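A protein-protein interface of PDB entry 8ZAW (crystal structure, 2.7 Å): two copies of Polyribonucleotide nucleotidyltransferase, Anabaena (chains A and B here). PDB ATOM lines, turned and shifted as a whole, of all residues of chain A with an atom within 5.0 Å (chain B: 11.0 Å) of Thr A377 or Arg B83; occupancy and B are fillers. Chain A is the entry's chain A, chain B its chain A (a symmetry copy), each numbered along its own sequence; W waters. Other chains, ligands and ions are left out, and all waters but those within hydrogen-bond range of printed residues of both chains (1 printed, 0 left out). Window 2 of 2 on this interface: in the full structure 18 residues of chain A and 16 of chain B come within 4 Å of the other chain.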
ATOM      1  N   HIS A 360     -12.978 -15.080 -13.544  1.00  0.00           N
ATOM      2  CA  HIS A 360     -12.552 -14.395 -14.756  1.00  0.00           C
ATOM      3  C   HIS A 360     -11.042 -14.432 -14.918  1.00  0.00           C
ATOM      4  O   HIS A 360     -10.541 -14.373 -16.044  1.00  0.00           O
ATOM      5  CB  HIS A 360     -13.051 -12.954 -14.748  1.00  0.00           C
ATOM      6  CG  HIS A 360     -14.524 -12.825 -14.526  1.00  0.00           C
ATOM      7  ND1 HIS A 360     -15.127 -11.632 -14.196  1.00  0.00           N
ATOM      8  CD2 HIS A 360     -15.521 -13.734 -14.617  1.00  0.00           C
ATOM      9  CE1 HIS A 360     -16.431 -11.815 -14.075  1.00  0.00           C
ATOM     10  NE2 HIS A 360     -16.695 -13.085 -14.321  1.00  0.00           N
ATOM     11  N   ALA A 375      -7.444 -14.137  -7.688  1.00  0.00           N
ATOM     12  CA  ALA A 375      -8.671 -14.344  -8.432  1.00  0.00           C
ATOM     13  C   ALA A 375      -9.193 -12.992  -8.876  1.00  0.00           C
ATOM     14  O   ALA A 375      -9.179 -12.025  -8.110  1.00  0.00           O
ATOM     15  CB  ALA A 375      -9.714 -15.084  -7.597  1.00  0.00           C
ATOM     16  N   CYS A 376      -9.630 -12.926 -10.123  1.00  0.00           N
ATOM     17  CA  CYS A 376     -10.009 -11.673 -10.751  1.00  0.00           C
ATOM     18  C   CYS A 376     -11.479 -11.731 -11.132  1.00  0.00           C
ATOM     19  O   CYS A 376     -11.922 -12.684 -11.781  1.00  0.00           O
ATOM     20  CB  CYS A 376      -9.144 -11.402 -11.987  1.00  0.00           C
ATOM     21  SG  CYS A 376      -9.400  -9.776 -12.696  1.00  0.00           S
ATOM     22  N   THR A 377     -12.222 -10.710 -10.719  1.00  0.00           N
ATOM     23  CA  THR A 377     -13.619 -10.533 -11.084  1.00  0.00           C
ATOM     24  C   THR A 377     -13.797  -9.201 -11.813  1.00  0.00           C
ATOM     25  O   THR A 377     -13.261  -8.167 -11.384  1.00  0.00           O
ATOM     26  CB  THR A 377     -14.510 -10.576  -9.845  1.00  0.00           C
ATOM     27  OG1 THR A 377     -14.321 -11.821  -9.158  1.00  0.00           O
ATOM     28  CG2 THR A 377     -15.955 -10.454 -10.265  1.00  0.00           C
ATOM     29  N   LEU A 378     -14.542  -9.237 -12.916  1.00  0.00           N
ATOM     30  CA  LEU A 378     -14.909  -8.054 -13.683  1.00  0.00           C
ATOM     31  C   LEU A 378     -16.404  -7.812 -13.554  1.00  0.00           C
ATOM     32  O   LEU A 378     -17.198  -8.756 -13.602  1.00  0.00           O
ATOM     33  CB  LEU A 378     -14.526  -8.210 -15.156  1.00  0.00           C
ATOM     34  CG  LEU A 378     -13.048  -8.519 -15.388  1.00  0.00           C
ATOM     35  CD1 LEU A 378     -12.788  -8.804 -16.836  1.00  0.00           C
ATOM     36  CD2 LEU A 378     -12.172  -7.379 -14.896  1.00  0.00           C
ATOM     37  N   GLY A 379     -16.781  -6.550 -13.385  1.00  0.00           N
ATOM     38  CA  GLY A 379     -18.181  -6.222 -13.223  1.00  0.00           C
ATOM     39  C   GLY A 379     -18.625  -5.018 -14.017  1.00  0.00           C
ATOM     40  O   GLY A 379     -18.052  -4.701 -15.063  1.00  0.00           O
ATOM     41  N   VAL A 447     -15.381  -2.753 -13.511  1.00  0.00           N
ATOM     42  CA  VAL A 447     -14.844  -2.538 -12.181  1.00  0.00           C
ATOM     43  C   VAL A 447     -14.015  -3.768 -11.832  1.00  0.00           C
ATOM     44  O   VAL A 447     -14.446  -4.904 -12.043  1.00  0.00           O
ATOM     45  CB  VAL A 447     -15.963  -2.275 -11.158  1.00  0.00           C
ATOM     46  CG1 VAL A 447     -16.872  -1.142 -11.656  1.00  0.00           C
ATOM     47  CG2 VAL A 447     -16.736  -3.530 -10.783  1.00  0.00           C
ATOM     48  N   ILE A 448     -12.790  -3.554 -11.373  1.00  0.00           N
ATOM     49  CA  ILE A 448     -11.838  -4.650 -11.248  1.00  0.00           C
ATOM     50  C   ILE A 448     -11.685  -5.007  -9.786  1.00  0.00           C
ATOM     51  O   ILE A 448     -11.485  -4.132  -8.927  1.00  0.00           O
ATOM     52  CB  ILE A 448     -10.477  -4.297 -11.869  1.00  0.00           C
ATOM     53  CG1 ILE A 448     -10.675  -3.976 -13.350  1.00  0.00           C
ATOM     54  CG2 ILE A 448      -9.483  -5.440 -11.645  1.00  0.00           C
ATOM     55  CD1 ILE A 448      -9.407  -3.687 -14.083  1.00  0.00           C
ATOM     56  N   ARG A 449     -11.752  -6.305  -9.517  1.00  0.00           N
ATOM     57  CA  ARG A 449     -11.803  -6.856  -8.175  1.00  0.00           C
ATOM     58  C   ARG A 449     -10.823  -8.019  -8.092  1.00  0.00           C
ATOM     59  O   ARG A 449     -10.927  -8.977  -8.869  1.00  0.00           O
ATOM     60  CB  ARG A 449     -13.232  -7.302  -7.871  1.00  0.00           C
ATOM     61  CG  ARG A 449     -13.429  -7.986  -6.577  1.00  0.00           C
ATOM     62  CD  ARG A 449     -12.919  -7.183  -5.455  1.00  0.00           C
ATOM     63  NE  ARG A 449     -13.377  -7.736  -4.192  1.00  0.00           N
ATOM     64  CZ  ARG A 449     -12.840  -7.469  -3.016  1.00  0.00           C
ATOM     65  NH1 ARG A 449     -11.836  -6.610  -2.922  1.00  0.00           N
ATOM     66  NH2 ARG A 449     -13.338  -8.027  -1.921  1.00  0.00           N
ATOM     67  N   VAL A 451      -8.807 -10.778  -5.448  1.00  0.00           N
ATOM     68  CA  VAL A 451      -8.706 -11.412  -4.141  1.00  0.00           C
ATOM     69  C   VAL A 451      -7.464 -12.289  -4.145  1.00  0.00           C
ATOM     70  O   VAL A 451      -7.309 -13.147  -5.018  1.00  0.00           O
ATOM     71  CB  VAL A 451      -9.967 -12.235  -3.800  1.00  0.00           C
ATOM     72  CG1 VAL A 451      -9.830 -12.865  -2.425  1.00  0.00           C
ATOM     73  CG2 VAL A 451     -11.213 -11.364  -3.874  1.00  0.00           C
ATOM     74  N   TYR B  74     -15.496 -23.031   7.143  1.00  0.00           N
ATOM     75  CA  TYR B  74     -15.896 -23.064   5.744  1.00  0.00           C
ATOM     76  C   TYR B  74     -16.103 -21.637   5.261  1.00  0.00           C
ATOM     77  O   TYR B  74     -16.748 -20.837   5.939  1.00  0.00           O
ATOM     78  CB  TYR B  74     -17.175 -23.877   5.556  1.00  0.00           C
ATOM     79  CG  TYR B  74     -17.775 -23.747   4.178  1.00  0.00           C
ATOM     80  CD1 TYR B  74     -17.323 -24.534   3.133  1.00  0.00           C
ATOM     81  CD2 TYR B  74     -18.799 -22.828   3.919  1.00  0.00           C
ATOM     82  CE1 TYR B  74     -17.872 -24.421   1.859  1.00  0.00           C
ATOM     83  CE2 TYR B  74     -19.356 -22.706   2.658  1.00  0.00           C
ATOM     84  CZ  TYR B  74     -18.888 -23.508   1.624  1.00  0.00           C
ATOM     85  OH  TYR B  74     -19.426 -23.410   0.349  1.00  0.00           O
ATOM     86  N   GLU B  75     -15.559 -21.325   4.094  1.00  0.00           N
ATOM     87  CA  GLU B  75     -15.748 -20.032   3.466  1.00  0.00           C
ATOM     88  C   GLU B  75     -16.318 -20.220   2.063  1.00  0.00           C
ATOM     89  O   GLU B  75     -15.883 -21.098   1.320  1.00  0.00           O
ATOM     90  CB  GLU B  75     -14.434 -19.251   3.422  1.00  0.00           C
ATOM     91  CG  GLU B  75     -13.744 -19.129   4.772  1.00  0.00           C
ATOM     92  CD  GLU B  75     -14.489 -18.215   5.738  1.00  0.00           C
ATOM     93  OE1 GLU B  75     -15.336 -17.429   5.268  1.00  0.00           O
ATOM     94  OE2 GLU B  75     -14.241 -18.287   6.965  1.00  0.00           O
ATOM     95  N   GLU B  76     -17.311 -19.414   1.723  1.00  0.00           N
ATOM     96  CA  GLU B  76     -17.894 -19.363   0.385  1.00  0.00           C
ATOM     97  C   GLU B  76     -17.526 -18.026  -0.247  1.00  0.00           C
ATOM     98  O   GLU B  76     -18.196 -17.018  -0.017  1.00  0.00           O
ATOM     99  CB  GLU B  76     -19.409 -19.539   0.439  1.00  0.00           C
ATOM    100  CG  GLU B  76     -19.995 -20.050  -0.860  1.00  0.00           C
ATOM    101  CD  GLU B  76     -21.386 -20.649  -0.695  1.00  0.00           C
ATOM    102  OE1 GLU B  76     -22.391 -19.935  -0.957  1.00  0.00           O
ATOM    103  OE2 GLU B  76     -21.457 -21.833  -0.297  1.00  0.00           O
ATOM    104  N   ARG B  77     -16.473 -18.023  -1.055  1.00  0.00           N
ATOM    105  CA  ARG B  77     -15.987 -16.777  -1.632  1.00  0.00           C
ATOM    106  C   ARG B  77     -16.941 -16.238  -2.695  1.00  0.00           C
ATOM    107  O   ARG B  77     -17.598 -16.997  -3.411  1.00  0.00           O
ATOM    108  CB  ARG B  77     -14.591 -16.982  -2.228  1.00  0.00           C
ATOM    109  CG  ARG B  77     -13.548 -17.495  -1.234  1.00  0.00           C
ATOM    110  CD  ARG B  77     -13.194 -16.437  -0.207  1.00  0.00           C
ATOM    111  NE  ARG B  77     -12.015 -16.823   0.536  1.00  0.00           N
ATOM    112  CZ  ARG B  77     -11.870 -16.691   1.845  1.00  0.00           C
ATOM    113  NH1 ARG B  77     -12.831 -16.158   2.586  1.00  0.00           N
ATOM    114  NH2 ARG B  77     -10.746 -17.088   2.409  1.00  0.00           N
ATOM    115  N   LEU B  78     -17.004 -14.908  -2.801  1.00  0.00           N
ATOM    116  CA  LEU B  78     -17.897 -14.291  -3.778  1.00  0.00           C
ATOM    117  C   LEU B  78     -17.266 -14.187  -5.166  1.00  0.00           C
ATOM    118  O   LEU B  78     -17.986 -14.158  -6.170  1.00  0.00           O
ATOM    119  CB  LEU B  78     -18.343 -12.914  -3.284  1.00  0.00           C
ATOM    120  CG  LEU B  78     -19.723 -12.826  -2.592  1.00  0.00           C
ATOM    121  CD1 LEU B  78     -19.871 -13.788  -1.427  1.00  0.00           C
ATOM    122  CD2 LEU B  78     -19.932 -11.414  -2.109  1.00  0.00           C
ATOM    123  N   TYR B  79     -15.930 -14.151  -5.269  1.00  0.00           N
ATOM    124  CA  TYR B  79     -15.320 -14.242  -6.589  1.00  0.00           C
ATOM    125  C   TYR B  79     -15.625 -15.567  -7.266  1.00  0.00           C
ATOM    126  O   TYR B  79     -15.533 -15.660  -8.491  1.00  0.00           O
ATOM    127  CB  TYR B  79     -13.811 -14.025  -6.505  1.00  0.00           C
ATOM    128  CG  TYR B  79     -13.018 -15.051  -5.720  1.00  0.00           C
ATOM    129  CD1 TYR B  79     -12.800 -16.333  -6.220  1.00  0.00           C
ATOM    130  CD2 TYR B  79     -12.441 -14.720  -4.492  1.00  0.00           C
ATOM    131  CE1 TYR B  79     -12.062 -17.260  -5.511  1.00  0.00           C
ATOM    132  CE2 TYR B  79     -11.703 -15.639  -3.777  1.00  0.00           C
ATOM    133  CZ  TYR B  79     -11.520 -16.913  -4.285  1.00  0.00           C
ATOM    134  OH  TYR B  79     -10.776 -17.832  -3.565  1.00  0.00           O
ATOM    135  N   ALA B  80     -15.987 -16.595  -6.497  1.00  0.00           N
ATOM    136  CA  ALA B  80     -16.276 -17.900  -7.083  1.00  0.00           C
ATOM    137  C   ALA B  80     -17.430 -17.846  -8.079  1.00  0.00           C
ATOM    138  O   ALA B  80     -17.541 -18.740  -8.922  1.00  0.00           O
ATOM    139  CB  ALA B  80     -16.573 -18.913  -5.972  1.00  0.00           C
ATOM    140  N   ALA B  81     -18.264 -16.801  -8.013  1.00  0.00           N
ATOM    141  CA  ALA B  81     -19.428 -16.653  -8.874  1.00  0.00           C
ATOM    142  C   ALA B  81     -19.540 -15.278  -9.537  1.00  0.00           C
ATOM    143  O   ALA B  81     -20.548 -15.026 -10.217  1.00  0.00           O
ATOM    144  CB  ALA B  81     -20.697 -16.920  -8.063  1.00  0.00           C
ATOM    145  N   GLY B  82     -18.549 -14.388  -9.360  1.00  0.00           N
ATOM    146  CA  GLY B  82     -18.715 -12.958  -9.605  1.00  0.00           C
ATOM    147  C   GLY B  82     -18.884 -12.138  -8.329  1.00  0.00           C
ATOM    148  O   GLY B  82     -19.962 -12.115  -7.719  1.00  0.00           O
ATOM    149  N   ARG B  83     -17.824 -11.439  -7.914  1.00  0.00           N
ATOM    150  CA  ARG B  83     -17.766 -10.779  -6.609  1.00  0.00           C
ATOM    151  C   ARG B  83     -18.219  -9.329  -6.715  1.00  0.00           C
ATOM    152  O   ARG B  83     -17.755  -8.589  -7.592  1.00  0.00           O
ATOM    153  CB  ARG B  83     -16.339 -10.837  -6.045  1.00  0.00           C
ATOM    154  CG  ARG B  83     -16.179 -10.241  -4.633  1.00  0.00           C
ATOM    155  CD  ARG B  83     -14.841 -10.629  -3.962  1.00  0.00           C
ATOM    156  NE  ARG B  83     -14.938 -11.908  -3.246  1.00  0.00           N
ATOM    157  CZ  ARG B  83     -14.345 -12.179  -2.083  1.00  0.00           C
ATOM    158  NH1 ARG B  83     -13.611 -11.256  -1.463  1.00  0.00           N
ATOM    159  NH2 ARG B  83     -14.503 -13.374  -1.525  1.00  0.00           N
ATOM    160  N   ILE B  84     -19.107  -8.922  -5.812  1.00  0.00           N
ATOM    161  CA  ILE B  84     -19.640  -7.563  -5.825  1.00  0.00           C
ATOM    162  C   ILE B  84     -19.448  -6.969  -4.437  1.00  0.00           C
ATOM    163  O   ILE B  84     -19.322  -7.703  -3.447  1.00  0.00           O
ATOM    164  CB  ILE B  84     -21.133  -7.525  -6.252  1.00  0.00           C
ATOM    165  CG1 ILE B  84     -22.067  -8.086  -5.180  1.00  0.00           C
ATOM    166  CG2 ILE B  84     -21.366  -8.450  -7.439  1.00  0.00           C
ATOM    167  CD1 ILE B  84     -23.504  -7.733  -5.462  1.00  0.00           C
ATOM    168  N   PRO B  85     -19.403  -5.629  -4.327  1.00  0.00           N
ATOM    169  CA  PRO B  85     -19.344  -5.026  -2.993  1.00  0.00           C
ATOM    170  C   PRO B  85     -20.719  -4.910  -2.349  1.00  0.00           C
ATOM    171  O   PRO B  85     -21.638  -5.586  -2.812  1.00  0.00           O
ATOM    172  CB  PRO B  85     -18.757  -3.642  -3.259  1.00  0.00           C
ATOM    173  CG  PRO B  85     -19.202  -3.316  -4.636  1.00  0.00           C
ATOM    174  CD  PRO B  85     -19.204  -4.623  -5.389  1.00  0.00           C
ATOM    175  N   THR B  99     -23.189 -19.914   5.802  1.00  0.00           N
ATOM    176  CA  THR B  99     -21.865 -20.524   5.841  1.00  0.00           C
ATOM    177  C   THR B  99     -21.608 -21.213   7.173  1.00  0.00           C
ATOM    178  O   THR B  99     -20.797 -22.142   7.235  1.00  0.00           O
ATOM    179  CB  THR B  99     -20.786 -19.480   5.604  1.00  0.00           C
ATOM    180  OG1 THR B  99     -20.690 -18.636   6.764  1.00  0.00           O
ATOM    181  CG2 THR B  99     -21.131 -18.647   4.380  1.00  0.00           C
ATOM    182  N   LEU B 127     -12.361 -23.711   1.599  1.00  0.00           N
ATOM    183  CA  LEU B 127     -12.718 -22.528   0.818  1.00  0.00           C
ATOM    184  C   LEU B 127     -13.346 -22.970  -0.493  1.00  0.00           C
ATOM    185  O   LEU B 127     -12.699 -23.650  -1.294  1.00  0.00           O
ATOM    186  CB  LEU B 127     -11.504 -21.648   0.517  1.00  0.00           C
ATOM    187  CG  LEU B 127     -10.543 -21.226   1.614  1.00  0.00           C
ATOM    188  CD1 LEU B 127      -9.346 -20.542   0.962  1.00  0.00           C
ATOM    189  CD2 LEU B 127     -11.225 -20.316   2.611  1.00  0.00           C
ATOM    190  N   THR B 128     -14.584 -22.563  -0.728  1.00  0.00           N
ATOM    191  CA  THR B 128     -15.189 -22.762  -2.034  1.00  0.00           C
ATOM    192  C   THR B 128     -14.679 -21.668  -2.957  1.00  0.00           C
ATOM    193  O   THR B 128     -14.846 -20.475  -2.672  1.00  0.00           O
ATOM    194  CB  THR B 128     -16.715 -22.737  -1.957  1.00  0.00           C
ATOM    195  OG1 THR B 128     -17.187 -23.749  -1.057  1.00  0.00           O
ATOM    196  CG2 THR B 128     -17.313 -22.972  -3.323  1.00  0.00           C
ATOM    197  N   MET B 129     -14.055 -22.073  -4.063  1.00  0.00           N
ATOM    198  CA  MET B 129     -13.380 -21.150  -4.958  1.00  0.00           C
ATOM    199  C   MET B 129     -14.000 -21.062  -6.346  1.00  0.00           C
ATOM    200  O   MET B 129     -13.577 -20.209  -7.136  1.00  0.00           O
ATOM    201  CB  MET B 129     -11.910 -21.541  -5.068  1.00  0.00           C
ATOM    202  CG  MET B 129     -11.278 -21.738  -3.703  1.00  0.00           C
ATOM    203  SD  MET B 129      -9.518 -22.088  -3.803  1.00  0.00           S
ATOM    204  CE  MET B 129      -8.893 -20.886  -2.638  1.00  0.00           C
ATOM    205  N   SER B 130     -14.984 -21.906  -6.663  1.00  0.00           N
ATOM    206  CA  SER B 130     -15.783 -21.761  -7.876  1.00  0.00           C
ATOM    207  C   SER B 130     -17.106 -22.477  -7.664  1.00  0.00           C
ATOM    208  O   SER B 130     -17.119 -23.632  -7.220  1.00  0.00           O
ATOM    209  CB  SER B 130     -15.062 -22.317  -9.117  1.00  0.00           C
ATOM    210  OG  SER B 130     -15.800 -22.014 -10.302  1.00  0.00           O
ATOM    211  N   MET B 131     -18.209 -21.774  -7.936  1.00  0.00           N
ATOM    212  CA  MET B 131     -19.535 -22.374  -7.973  1.00  0.00           C
ATOM    213  C   MET B 131     -19.926 -22.582  -9.427  1.00  0.00           C
ATOM    214  O   MET B 131     -20.109 -21.611 -10.169  1.00  0.00           O
ATOM    215  CB  MET B 131     -20.597 -21.525  -7.278  1.00  0.00           C
ATOM    216  CG  MET B 131     -20.776 -21.774  -5.800  1.00  0.00           C
ATOM    217  SD  MET B 131     -19.507 -20.970  -4.854  1.00  0.00           S
ATOM    218  CE  MET B 131     -19.946 -19.274  -5.189  1.00  0.00           C
HETATM  219  O   HOH W   1     -14.625 -13.945 -10.894  1.00  0.00           O
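N of Ala A375 lies within hydrogen-bond range of O of Val A451, 2.9 Å away. O of Arg A449 sits at hydrogen-bond distance from N of Thr A377 (2.8 Å). The backbone NH (N) of Arg B83 lies within hydrogen-bond range of the backbone carbonyl oxygen (O) of Leu B78, at 3.2 Å.
Printed residues of chain B within 4 Å of Ala A375: Tyr B79 (3.6 Å). No residue of chain B comes within 4 Å of Cys A376. Of the printed residues of chain B, Thr A377 touches Tyr B79 (3.5 Å), Gly B82 (3.8 Å) and Arg B83 (3.2 Å). No residue of chain B comes within 4 Å of Leu A378. No residue of chain B comes within 4 Å of Ile A448. Of the printed residues of chain B, Val A451 touches Tyr B79 and Arg B83. Of the printed residues of chain A, Tyr B79 touches Ala A375, Thr A377 and Val A451. Ala B80 touches none of the printed residues of chain A. Printed residues of chain A within 4 Å of Gly B82: Thr A377 (3.8 Å). Arg B83 touches just these residues of chain A: Thr A377, Arg A449 and Val A451. The nearest residue of chain B that does not touch Thr A377 is Leu B78 (5.3 Å). The nearest printed residue of chain A that does not touch Gly B82 is His A360 (5.1 Å).
Among the printed residues, merely in contact across the chains: Thr A377 with Arg B83 (3.2 Å), Val A451 with Arg B83 (3.4 Å), Thr A377 with Tyr B79 (3.5 Å), Val A451 with Tyr B79 (3.6 Å), Ala A375 with Tyr B79 (3.6 Å) and Thr A377 with Gly B82 (3.8 Å).
Water W1 lies within hydrogen-bond range of OG1 of Thr A377 (2.8 Å), O of Tyr B79 (3.1 Å), O of Cys A376 (3.1 Å) and N of His A360 (3.3 Å).
Of the 10 printed residues of chain A, 4 touch a printed residue of chain B. Hydrophobic or aromatic side chains of chain A within 4 Å of the printed part of chain B: Ala A375 and Val A451. Of the 18 printed residues of chain B, 3 touch a printed residue of chain A. Among the printed residues, 7 pairs touch across the chains.
The guanidinium group of Arg A449 sits close to the guanidinium group of Arg B83.
No position is printed for both chains. Of the 7 pairs that touch across the chains among the printed residues, none has its exchanged pair printed and touching as well.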
